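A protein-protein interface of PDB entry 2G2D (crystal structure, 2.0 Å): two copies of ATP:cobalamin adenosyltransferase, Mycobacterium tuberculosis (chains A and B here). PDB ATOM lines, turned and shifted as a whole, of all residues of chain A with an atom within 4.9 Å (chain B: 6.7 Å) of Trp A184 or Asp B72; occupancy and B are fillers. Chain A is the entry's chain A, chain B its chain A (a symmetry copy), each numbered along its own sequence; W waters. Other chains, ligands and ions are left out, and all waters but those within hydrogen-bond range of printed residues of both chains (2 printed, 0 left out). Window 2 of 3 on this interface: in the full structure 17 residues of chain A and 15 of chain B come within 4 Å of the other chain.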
ATOM      1  N   SER A 116      29.936 -10.418  -8.408  1.00  0.00           N
ATOM      2  CA  SER A 116      28.563 -10.403  -8.909  1.00  0.00           C
ATOM      3  C   SER A 116      28.546 -11.198 -10.198  1.00  0.00           C
ATOM      4  O   SER A 116      29.573 -11.741 -10.617  1.00  0.00           O
ATOM      5  CB  SER A 116      28.062  -8.984  -9.199  1.00  0.00           C
ATOM      6  OG  SER A 116      26.666  -9.016  -9.507  1.00  0.00           O
ATOM      7  N   PHE A 117      27.379 -11.295 -10.815  1.00  0.00           N
ATOM      8  CA  PHE A 117      27.279 -12.016 -12.071  1.00  0.00           C
ATOM      9  C   PHE A 117      27.877 -11.134 -13.155  1.00  0.00           C
ATOM     10  O   PHE A 117      27.781  -9.902 -13.097  1.00  0.00           O
ATOM     11  CB  PHE A 117      25.827 -12.339 -12.399  1.00  0.00           C
ATOM     12  CG  PHE A 117      25.190 -13.289 -11.427  1.00  0.00           C
ATOM     13  CD1 PHE A 117      24.717 -12.836 -10.201  1.00  0.00           C
ATOM     14  CD2 PHE A 117      25.068 -14.637 -11.743  1.00  0.00           C
ATOM     15  CE1 PHE A 117      24.126 -13.707  -9.298  1.00  0.00           C
ATOM     16  CE2 PHE A 117      24.476 -15.527 -10.848  1.00  0.00           C
ATOM     17  CZ  PHE A 117      24.003 -15.061  -9.622  1.00  0.00           C
ATOM     18  N   LEU A 119      28.261  -9.523 -16.908  1.00  0.00           N
ATOM     19  CA  LEU A 119      27.453  -9.158 -18.067  1.00  0.00           C
ATOM     20  C   LEU A 119      28.439  -9.287 -19.232  1.00  0.00           C
ATOM     21  O   LEU A 119      29.620  -8.995 -19.075  1.00  0.00           O
ATOM     22  CB  LEU A 119      26.913  -7.728 -17.940  1.00  0.00           C
ATOM     23  CG  LEU A 119      25.912  -7.512 -16.789  1.00  0.00           C
ATOM     24  CD1 LEU A 119      25.366  -6.077 -16.831  1.00  0.00           C
ATOM     25  CD2 LEU A 119      24.765  -8.525 -16.908  1.00  0.00           C
ATOM     26  N   VAL A 182      32.385  -6.691 -16.548  1.00  0.00           N
ATOM     27  CA  VAL A 182      31.219  -5.816 -16.457  1.00  0.00           C
ATOM     28  C   VAL A 182      30.286  -6.602 -15.545  1.00  0.00           C
ATOM     29  O   VAL A 182      29.955  -7.743 -15.851  1.00  0.00           O
ATOM     30  CB  VAL A 182      30.559  -5.617 -17.836  1.00  0.00           C
ATOM     31  CG1 VAL A 182      29.350  -4.680 -17.704  1.00  0.00           C
ATOM     32  CG2 VAL A 182      31.588  -5.016 -18.822  1.00  0.00           C
ATOM     33  N   LEU A 183      29.870  -6.009 -14.426  1.00  0.00           N
ATOM     34  CA  LEU A 183      29.014  -6.718 -13.464  1.00  0.00           C
ATOM     35  C   LEU A 183      27.553  -6.287 -13.362  1.00  0.00           C
ATOM     36  O   LEU A 183      27.222  -5.104 -13.472  1.00  0.00           O
ATOM     37  CB  LEU A 183      29.619  -6.609 -12.060  1.00  0.00           C
ATOM     38  CG  LEU A 183      31.098  -6.972 -11.900  1.00  0.00           C
ATOM     39  CD1 LEU A 183      31.520  -6.675 -10.470  1.00  0.00           C
ATOM     40  CD2 LEU A 183      31.326  -8.433 -12.249  1.00  0.00           C
ATOM     41  N   TRP A 184      26.694  -7.268 -13.110  1.00  0.00           N
ATOM     42  CA  TRP A 184      25.265  -7.045 -12.937  1.00  0.00           C
ATOM     43  C   TRP A 184      25.062  -6.385 -11.574  1.00  0.00           C
ATOM     44  O   TRP A 184      25.830  -6.628 -10.636  1.00  0.00           O
ATOM     45  CB  TRP A 184      24.524  -8.382 -12.945  1.00  0.00           C
ATOM     46  CG  TRP A 184      23.094  -8.289 -12.534  1.00  0.00           C
ATOM     47  CD1 TRP A 184      22.056  -7.770 -13.260  1.00  0.00           C
ATOM     48  CD2 TRP A 184      22.532  -8.734 -11.293  1.00  0.00           C
ATOM     49  NE1 TRP A 184      20.877  -7.874 -12.546  1.00  0.00           N
ATOM     50  CE2 TRP A 184      21.144  -8.459 -11.337  1.00  0.00           C
ATOM     51  CE3 TRP A 184      23.068  -9.342 -10.148  1.00  0.00           C
ATOM     52  CZ2 TRP A 184      20.286  -8.771 -10.279  1.00  0.00           C
ATOM     53  CZ3 TRP A 184      22.210  -9.654  -9.092  1.00  0.00           C
ATOM     54  CH2 TRP A 184      20.834  -9.366  -9.168  1.00  0.00           C
ATOM     55  N   ARG A 185      24.019  -5.569 -11.466  1.00  0.00           N
ATOM     56  CA  ARG A 185      23.702  -4.881 -10.216  1.00  0.00           C
ATOM     57  C   ARG A 185      22.213  -5.046  -9.903  1.00  0.00           C
ATOM     58  O   ARG A 185      21.359  -4.746 -10.746  1.00  0.00           O
ATOM     59  CB  ARG A 185      24.036  -3.398 -10.347  1.00  0.00           C
ATOM     60  CG  ARG A 185      25.474  -3.136 -10.743  1.00  0.00           C
ATOM     61  CD  ARG A 185      25.705  -1.656 -10.990  1.00  0.00           C
ATOM     62  NE  ARG A 185      27.106  -1.361 -11.277  1.00  0.00           N
ATOM     63  CZ  ARG A 185      27.566  -0.151 -11.579  1.00  0.00           C
ATOM     64  NH1 ARG A 185      26.732   0.880 -11.635  1.00  0.00           N
ATOM     65  NH2 ARG A 185      28.859   0.028 -11.822  1.00  0.00           N
ATOM     66  N   PRO A 186      21.882  -5.528  -8.691  1.00  0.00           N
ATOM     67  CA  PRO A 186      20.482  -5.724  -8.293  1.00  0.00           C
ATOM     68  C   PRO A 186      19.680  -4.453  -8.554  1.00  0.00           C
ATOM     69  O   PRO A 186      20.162  -3.354  -8.289  1.00  0.00           O
ATOM     70  CB  PRO A 186      20.585  -6.035  -6.801  1.00  0.00           C
ATOM     71  CG  PRO A 186      21.920  -6.687  -6.684  1.00  0.00           C
ATOM     72  CD  PRO A 186      22.785  -5.823  -7.567  1.00  0.00           C
ATOM     73  N   GLY A 187      18.467  -4.618  -9.076  1.00  0.00           N
ATOM     74  CA  GLY A 187      17.610  -3.482  -9.384  1.00  0.00           C
ATOM     75  C   GLY A 187      17.664  -2.371  -8.357  1.00  0.00           C
ATOM     76  O   GLY A 187      17.852  -1.204  -8.703  1.00  0.00           O
ATOM     77  N   ASN B  43      22.312 -10.077 -25.370  1.00  0.00           N
ATOM     78  CA  ASN B  43      23.084  -9.262 -24.441  1.00  0.00           C
ATOM     79  C   ASN B  43      24.535  -9.132 -24.906  1.00  0.00           C
ATOM     80  O   ASN B  43      25.123  -8.045 -24.814  1.00  0.00           O
ATOM     81  CB  ASN B  43      23.021  -9.851 -23.023  1.00  0.00           C
ATOM     82  CG  ASN B  43      23.204  -8.792 -21.942  1.00  0.00           C
ATOM     83  OD1 ASN B  43      23.489  -7.636 -22.244  1.00  0.00           O
ATOM     84  ND2 ASN B  43      23.038  -9.185 -20.674  1.00  0.00           N
ATOM     85  N   GLN B  65      22.360  -0.015 -19.094  1.00  0.00           N
ATOM     86  CA  GLN B  65      21.169  -0.322 -18.320  1.00  0.00           C
ATOM     87  C   GLN B  65      20.430  -1.468 -18.988  1.00  0.00           C
ATOM     88  O   GLN B  65      19.855  -2.333 -18.320  1.00  0.00           O
ATOM     89  CB  GLN B  65      20.241   0.891 -18.213  1.00  0.00           C
ATOM     90  CG  GLN B  65      18.953   0.602 -17.428  1.00  0.00           C
ATOM     91  CD  GLN B  65      19.221   0.125 -15.999  1.00  0.00           C
ATOM     92  OE1 GLN B  65      20.038   0.706 -15.283  1.00  0.00           O
ATOM     93  NE2 GLN B  65      18.523  -0.928 -15.581  1.00  0.00           N
ATOM     94  N   GLN B  67      21.796  -3.855 -20.700  1.00  0.00           N
ATOM     95  CA  GLN B  67      22.515  -5.123 -20.447  1.00  0.00           C
ATOM     96  C   GLN B  67      22.071  -5.676 -19.098  1.00  0.00           C
ATOM     97  O   GLN B  67      21.862  -6.877 -18.937  1.00  0.00           O
ATOM     98  CB  GLN B  67      24.026  -4.905 -20.437  1.00  0.00           C
ATOM     99  CG  GLN B  67      24.610  -4.608 -21.817  1.00  0.00           C
ATOM    100  CD  GLN B  67      26.045  -5.087 -21.948  1.00  0.00           C
ATOM    101  OE1 GLN B  67      26.959  -4.487 -21.403  1.00  0.00           O
ATOM    102  NE2 GLN B  67      26.243  -6.190 -22.666  1.00  0.00           N
ATOM    103  N   ASN B  68      21.905  -4.781 -18.133  1.00  0.00           N
ATOM    104  CA  ASN B  68      21.455  -5.180 -16.801  1.00  0.00           C
ATOM    105  C   ASN B  68      20.027  -5.743 -16.879  1.00  0.00           C
ATOM    106  O   ASN B  68      19.714  -6.744 -16.223  1.00  0.00           O
ATOM    107  CB  ASN B  68      21.523  -3.967 -15.859  1.00  0.00           C
ATOM    108  CG  ASN B  68      21.647  -4.367 -14.411  1.00  0.00           C
ATOM    109  OD1 ASN B  68      20.647  -4.568 -13.718  1.00  0.00           O
ATOM    110  ND2 ASN B  68      22.882  -4.513 -13.948  1.00  0.00           N
ATOM    111  N   ASP B  69      19.160  -5.104 -17.673  1.00  0.00           N
ATOM    112  CA  ASP B  69      17.776  -5.567 -17.835  1.00  0.00           C
ATOM    113  C   ASP B  69      17.719  -6.929 -18.527  1.00  0.00           C
ATOM    114  O   ASP B  69      16.860  -7.762 -18.213  1.00  0.00           O
ATOM    115  CB  ASP B  69      16.941  -4.608 -18.700  1.00  0.00           C
ATOM    116  CG  ASP B  69      16.774  -3.219 -18.090  1.00  0.00           C
ATOM    117  OD1 ASP B  69      16.979  -3.037 -16.871  1.00  0.00           O
ATOM    118  OD2 ASP B  69      16.417  -2.305 -18.863  1.00  0.00           O
ATOM    119  N   LEU B  70      18.597  -7.137 -19.509  1.00  0.00           N
ATOM    120  CA  LEU B  70      18.608  -8.412 -20.232  1.00  0.00           C
ATOM    121  C   LEU B  70      19.015  -9.584 -19.321  1.00  0.00           C
ATOM    122  O   LEU B  70      18.582 -10.725 -19.525  1.00  0.00           O
ATOM    123  CB  LEU B  70      19.519  -8.321 -21.471  1.00  0.00           C
ATOM    124  CG  LEU B  70      18.904  -7.513 -22.632  1.00  0.00           C
ATOM    125  CD1 LEU B  70      19.889  -7.375 -23.763  1.00  0.00           C
ATOM    126  CD2 LEU B  70      17.629  -8.209 -23.144  1.00  0.00           C
ATOM    127  N   PHE B  71      19.846  -9.308 -18.322  1.00  0.00           N
ATOM    128  CA  PHE B  71      20.240 -10.354 -17.366  1.00  0.00           C
ATOM    129  C   PHE B  71      18.959 -10.740 -16.622  1.00  0.00           C
ATOM    130  O   PHE B  71      18.625 -11.917 -16.461  1.00  0.00           O
ATOM    131  CB  PHE B  71      21.253  -9.805 -16.363  1.00  0.00           C
ATOM    132  CG  PHE B  71      21.682 -10.811 -15.327  1.00  0.00           C
ATOM    133  CD1 PHE B  71      22.750 -11.665 -15.566  1.00  0.00           C
ATOM    134  CD2 PHE B  71      20.985 -10.922 -14.122  1.00  0.00           C
ATOM    135  CE1 PHE B  71      23.118 -12.618 -14.624  1.00  0.00           C
ATOM    136  CE2 PHE B  71      21.343 -11.873 -13.169  1.00  0.00           C
ATOM    137  CZ  PHE B  71      22.410 -12.725 -13.419  1.00  0.00           C
ATOM    138  N   ASP B  72      18.231  -9.718 -16.181  1.00  0.00           N
ATOM    139  CA  ASP B  72      16.973  -9.911 -15.481  1.00  0.00           C
ATOM    140  C   ASP B  72      15.988 -10.693 -16.356  1.00  0.00           C
ATOM    141  O   ASP B  72      15.298 -11.596 -15.874  1.00  0.00           O
ATOM    142  CB  ASP B  72      16.365  -8.545 -15.104  1.00  0.00           C
ATOM    143  CG  ASP B  72      17.204  -7.783 -14.085  1.00  0.00           C
ATOM    144  OD1 ASP B  72      18.234  -8.305 -13.614  1.00  0.00           O
ATOM    145  OD2 ASP B  72      16.837  -6.649 -13.747  1.00  0.00           O
ATOM    146  N   ALA B  73      15.917 -10.348 -17.645  1.00  0.00           N
ATOM    147  CA  ALA B  73      14.997 -11.033 -18.549  1.00  0.00           C
ATOM    148  C   ALA B  73      15.342 -12.518 -18.624  1.00  0.00           C
ATOM    149  O   ALA B  73      14.445 -13.371 -18.628  1.00  0.00           O
ATOM    150  CB  ALA B  73      15.057 -10.411 -19.949  1.00  0.00           C
ATOM    151  N   GLY B  74      16.640 -12.812 -18.679  1.00  0.00           N
ATOM    152  CA  GLY B  74      17.108 -14.193 -18.745  1.00  0.00           C
ATOM    153  C   GLY B  74      16.738 -14.952 -17.480  1.00  0.00           C
ATOM    154  O   GLY B  74      16.194 -16.050 -17.555  1.00  0.00           O
ATOM    155  N   ALA B  75      17.027 -14.363 -16.320  1.00  0.00           N
ATOM    156  CA  ALA B  75      16.701 -14.982 -15.030  1.00  0.00           C
ATOM    157  C   ALA B  75      15.196 -15.272 -14.928  1.00  0.00           C
ATOM    158  O   ALA B  75      14.788 -16.328 -14.463  1.00  0.00           O
ATOM    159  CB  ALA B  75      17.139 -14.065 -13.882  1.00  0.00           C
ATOM    160  N   ASP B  76      14.383 -14.323 -15.379  1.00  0.00           N
ATOM    161  CA  ASP B  76      12.919 -14.432 -15.373  1.00  0.00           C
ATOM    162  C   ASP B  76      12.482 -15.615 -16.247  1.00  0.00           C
ATOM    163  O   ASP B  76      11.771 -16.508 -15.803  1.00  0.00           O
ATOM    164  CB  ASP B  76      12.337 -13.132 -15.942  1.00  0.00           C
ATOM    165  CG  ASP B  76      10.829 -13.035 -15.812  1.00  0.00           C
ATOM    166  OD1 ASP B  76      10.123 -14.066 -15.836  1.00  0.00           O
ATOM    167  OD2 ASP B  76      10.350 -11.892 -15.712  1.00  0.00           O
ATOM    168  N   LEU B  77      12.918 -15.610 -17.501  1.00  0.00           N
ATOM    169  CA  LEU B  77      12.566 -16.669 -18.440  1.00  0.00           C
ATOM    170  C   LEU B  77      12.987 -18.066 -17.974  1.00  0.00           C
ATOM    171  O   LEU B  77      12.264 -19.048 -18.181  1.00  0.00           O
ATOM    172  CB  LEU B  77      13.191 -16.361 -19.814  1.00  0.00           C
ATOM    173  CG  LEU B  77      12.554 -15.190 -20.575  1.00  0.00           C
ATOM    174  CD1 LEU B  77      13.482 -14.679 -21.693  1.00  0.00           C
ATOM    175  CD2 LEU B  77      11.219 -15.659 -21.149  1.00  0.00           C
ATOM    176  N   LEU B  90      13.078 -12.098  -9.335  1.00  0.00           N
ATOM    177  CA  LEU B  90      13.911 -11.358 -10.273  1.00  0.00           C
ATOM    178  C   LEU B  90      13.093 -11.518 -11.542  1.00  0.00           C
ATOM    179  O   LEU B  90      13.257 -12.475 -12.303  1.00  0.00           O
ATOM    180  CB  LEU B  90      15.309 -11.982 -10.418  1.00  0.00           C
ATOM    181  CG  LEU B  90      16.237 -11.166 -11.339  1.00  0.00           C
ATOM    182  CD1 LEU B  90      16.168  -9.686 -10.966  1.00  0.00           C
ATOM    183  CD2 LEU B  90      17.664 -11.681 -11.237  1.00  0.00           C
ATOM    184  N   ARG B  91      12.170 -10.582 -11.725  1.00  0.00           N
ATOM    185  CA  ARG B  91      11.251 -10.611 -12.841  1.00  0.00           C
ATOM    186  C   ARG B  91      11.221  -9.269 -13.551  1.00  0.00           C
ATOM    187  O   ARG B  91      11.396  -8.225 -12.925  1.00  0.00           O
ATOM    188  CB  ARG B  91       9.839 -10.921 -12.319  1.00  0.00           C
ATOM    189  CG  ARG B  91       9.686 -12.240 -11.561  1.00  0.00           C
ATOM    190  CD  ARG B  91       9.509 -13.410 -12.510  1.00  0.00           C
ATOM    191  NE  ARG B  91       9.323 -14.668 -11.794  1.00  0.00           N
ATOM    192  CZ  ARG B  91       9.612 -15.864 -12.303  1.00  0.00           C
ATOM    193  NH1 ARG B  91      10.101 -15.969 -13.538  1.00  0.00           N
ATOM    194  NH2 ARG B  91       9.432 -16.956 -11.571  1.00  0.00           N
ATOM    195  N   ILE B  92      11.017  -9.298 -14.860  1.00  0.00           N
ATOM    196  CA  ILE B  92      10.893  -8.060 -15.613  1.00  0.00           C
ATOM    197  C   ILE B  92       9.530  -7.515 -15.154  1.00  0.00           C
ATOM    198  O   ILE B  92       8.547  -8.267 -15.088  1.00  0.00           O
ATOM    199  CB  ILE B  92      10.845  -8.328 -17.157  1.00  0.00           C
ATOM    200  CG1 ILE B  92      12.227  -8.773 -17.665  1.00  0.00           C
ATOM    201  CG2 ILE B  92      10.382  -7.075 -17.907  1.00  0.00           C
ATOM    202  CD1 ILE B  92      13.327  -7.743 -17.472  1.00  0.00           C
ATOM    203  N   TYR B  96       9.908  -1.688 -16.485  1.00  0.00           N
ATOM    204  CA  TYR B  96      11.059  -1.842 -17.381  1.00  0.00           C
ATOM    205  C   TYR B  96      10.634  -1.422 -18.781  1.00  0.00           C
ATOM    206  O   TYR B  96      11.349  -0.705 -19.486  1.00  0.00           O
ATOM    207  CB  TYR B  96      11.504  -3.300 -17.459  1.00  0.00           C
ATOM    208  CG  TYR B  96      12.315  -3.815 -16.298  1.00  0.00           C
ATOM    209  CD1 TYR B  96      13.578  -4.362 -16.515  1.00  0.00           C
ATOM    210  CD2 TYR B  96      11.794  -3.852 -15.003  1.00  0.00           C
ATOM    211  CE1 TYR B  96      14.309  -4.948 -15.482  1.00  0.00           C
ATOM    212  CE2 TYR B  96      12.524  -4.439 -13.948  1.00  0.00           C
ATOM    213  CZ  TYR B  96      13.781  -4.988 -14.205  1.00  0.00           C
ATOM    214  OH  TYR B  96      14.509  -5.606 -13.202  1.00  0.00           O
ATOM    215  N   PRO B 158       8.933 -10.671 -20.192  1.00  0.00           N
ATOM    216  CA  PRO B 158      10.244 -10.683 -20.862  1.00  0.00           C
ATOM    217  C   PRO B 158      10.084 -10.484 -22.394  1.00  0.00           C
ATOM    218  O   PRO B 158      10.811  -9.695 -23.016  1.00  0.00           O
ATOM    219  CB  PRO B 158      10.801 -12.052 -20.488  1.00  0.00           C
ATOM    220  CG  PRO B 158      10.255 -12.242 -19.064  1.00  0.00           C
ATOM    221  CD  PRO B 158       8.809 -11.779 -19.225  1.00  0.00           C
HETATM  222  O   HOH W   1      17.969  -6.251 -11.203  1.00  0.00           O
HETATM  223  O   HOH W   2      25.224  -3.335 -14.372  1.00  0.00           O
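The side-chain carboxylate (OD1) of Asp B72 sits at hydrogen-bond distance from the indole nitrogen (NE1) of Trp A184, at 2.9 Å. The backbone NH (N) of Arg A185 lies close to the side-chain amide nitrogen (ND2) of Asn B68 (2.9 Å).
NE2 of Gln B67 is in hydrogen-bond range of O of Asn B43, 3.1 Å away. O of Phe A117 lies within hydrogen-bond range of N of Trp A184 (2.8 Å). OH of Tyr B96 lies within hydrogen-bond range of OD2 of Asp B72, 2.6 Å away. O of Val A182 is in hydrogen-bond range of N of Leu A119 (2.7 Å). The side-chain hydroxyl (OG) of Ser A116 lies within hydrogen-bond range of the backbone carbonyl oxygen (O) of Trp A184 (2.8 Å).
Among the printed residues, pairs that only touch across the chains: Trp A184 with Asn B68 (3.4 Å), Trp A184 with Phe B71 (3.4 Å), Phe A117 with Phe B71 (3.5 Å), Leu A119 with Phe B71 (3.8 Å), Leu A119 with Gln B67 (3.9 Å) and Leu A119 with Asn B68 (3.9 Å).
Of the printed residues of chain B, Phe A117 touches Phe B71 (3.5 Å). Printed residues of chain B within 4 Å of Leu A119: Gln B67 (3.9 Å), Asn B68 (3.9 Å) and Phe B71 (3.8 Å). Trp A184 touches three residues of chain B. Printed residues of chain A within 4 Å of Phe B71: Phe A117 (3.5 Å), Leu A119 (3.8 Å) and Trp A184 (3.4 Å). Of chain A, only Trp A184 comes within 4 Å of Asp B72. Ala B73 touches none of the printed residues of chain A. Ala B75 touches none of the printed residues of chain A. The nearest printed residue of chain A that does not touch Asn B68 is Leu A183 (4.4 Å).
Hydrophobic or aromatic side chains of chain B that line the printed part of chain A: Phe B71. Along chain B the printed residues that touch a printed residue of chain A span positions 67 to 72. Of the 9 printed residues of chain A, 4 touch a printed residue of chain B.
No position is printed for both chains. Of the 8 pairs that touch across the chains among the printed residues, none has its exchanged pair printed and touching as well.
Water W2 lies within hydrogen-bond range of ND2 of Asn B68 and O of Leu A183. Water W1 bridges the backbone NH (N) of Gly A187 and the side-chain carboxylate (OD2) of Asp B72.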
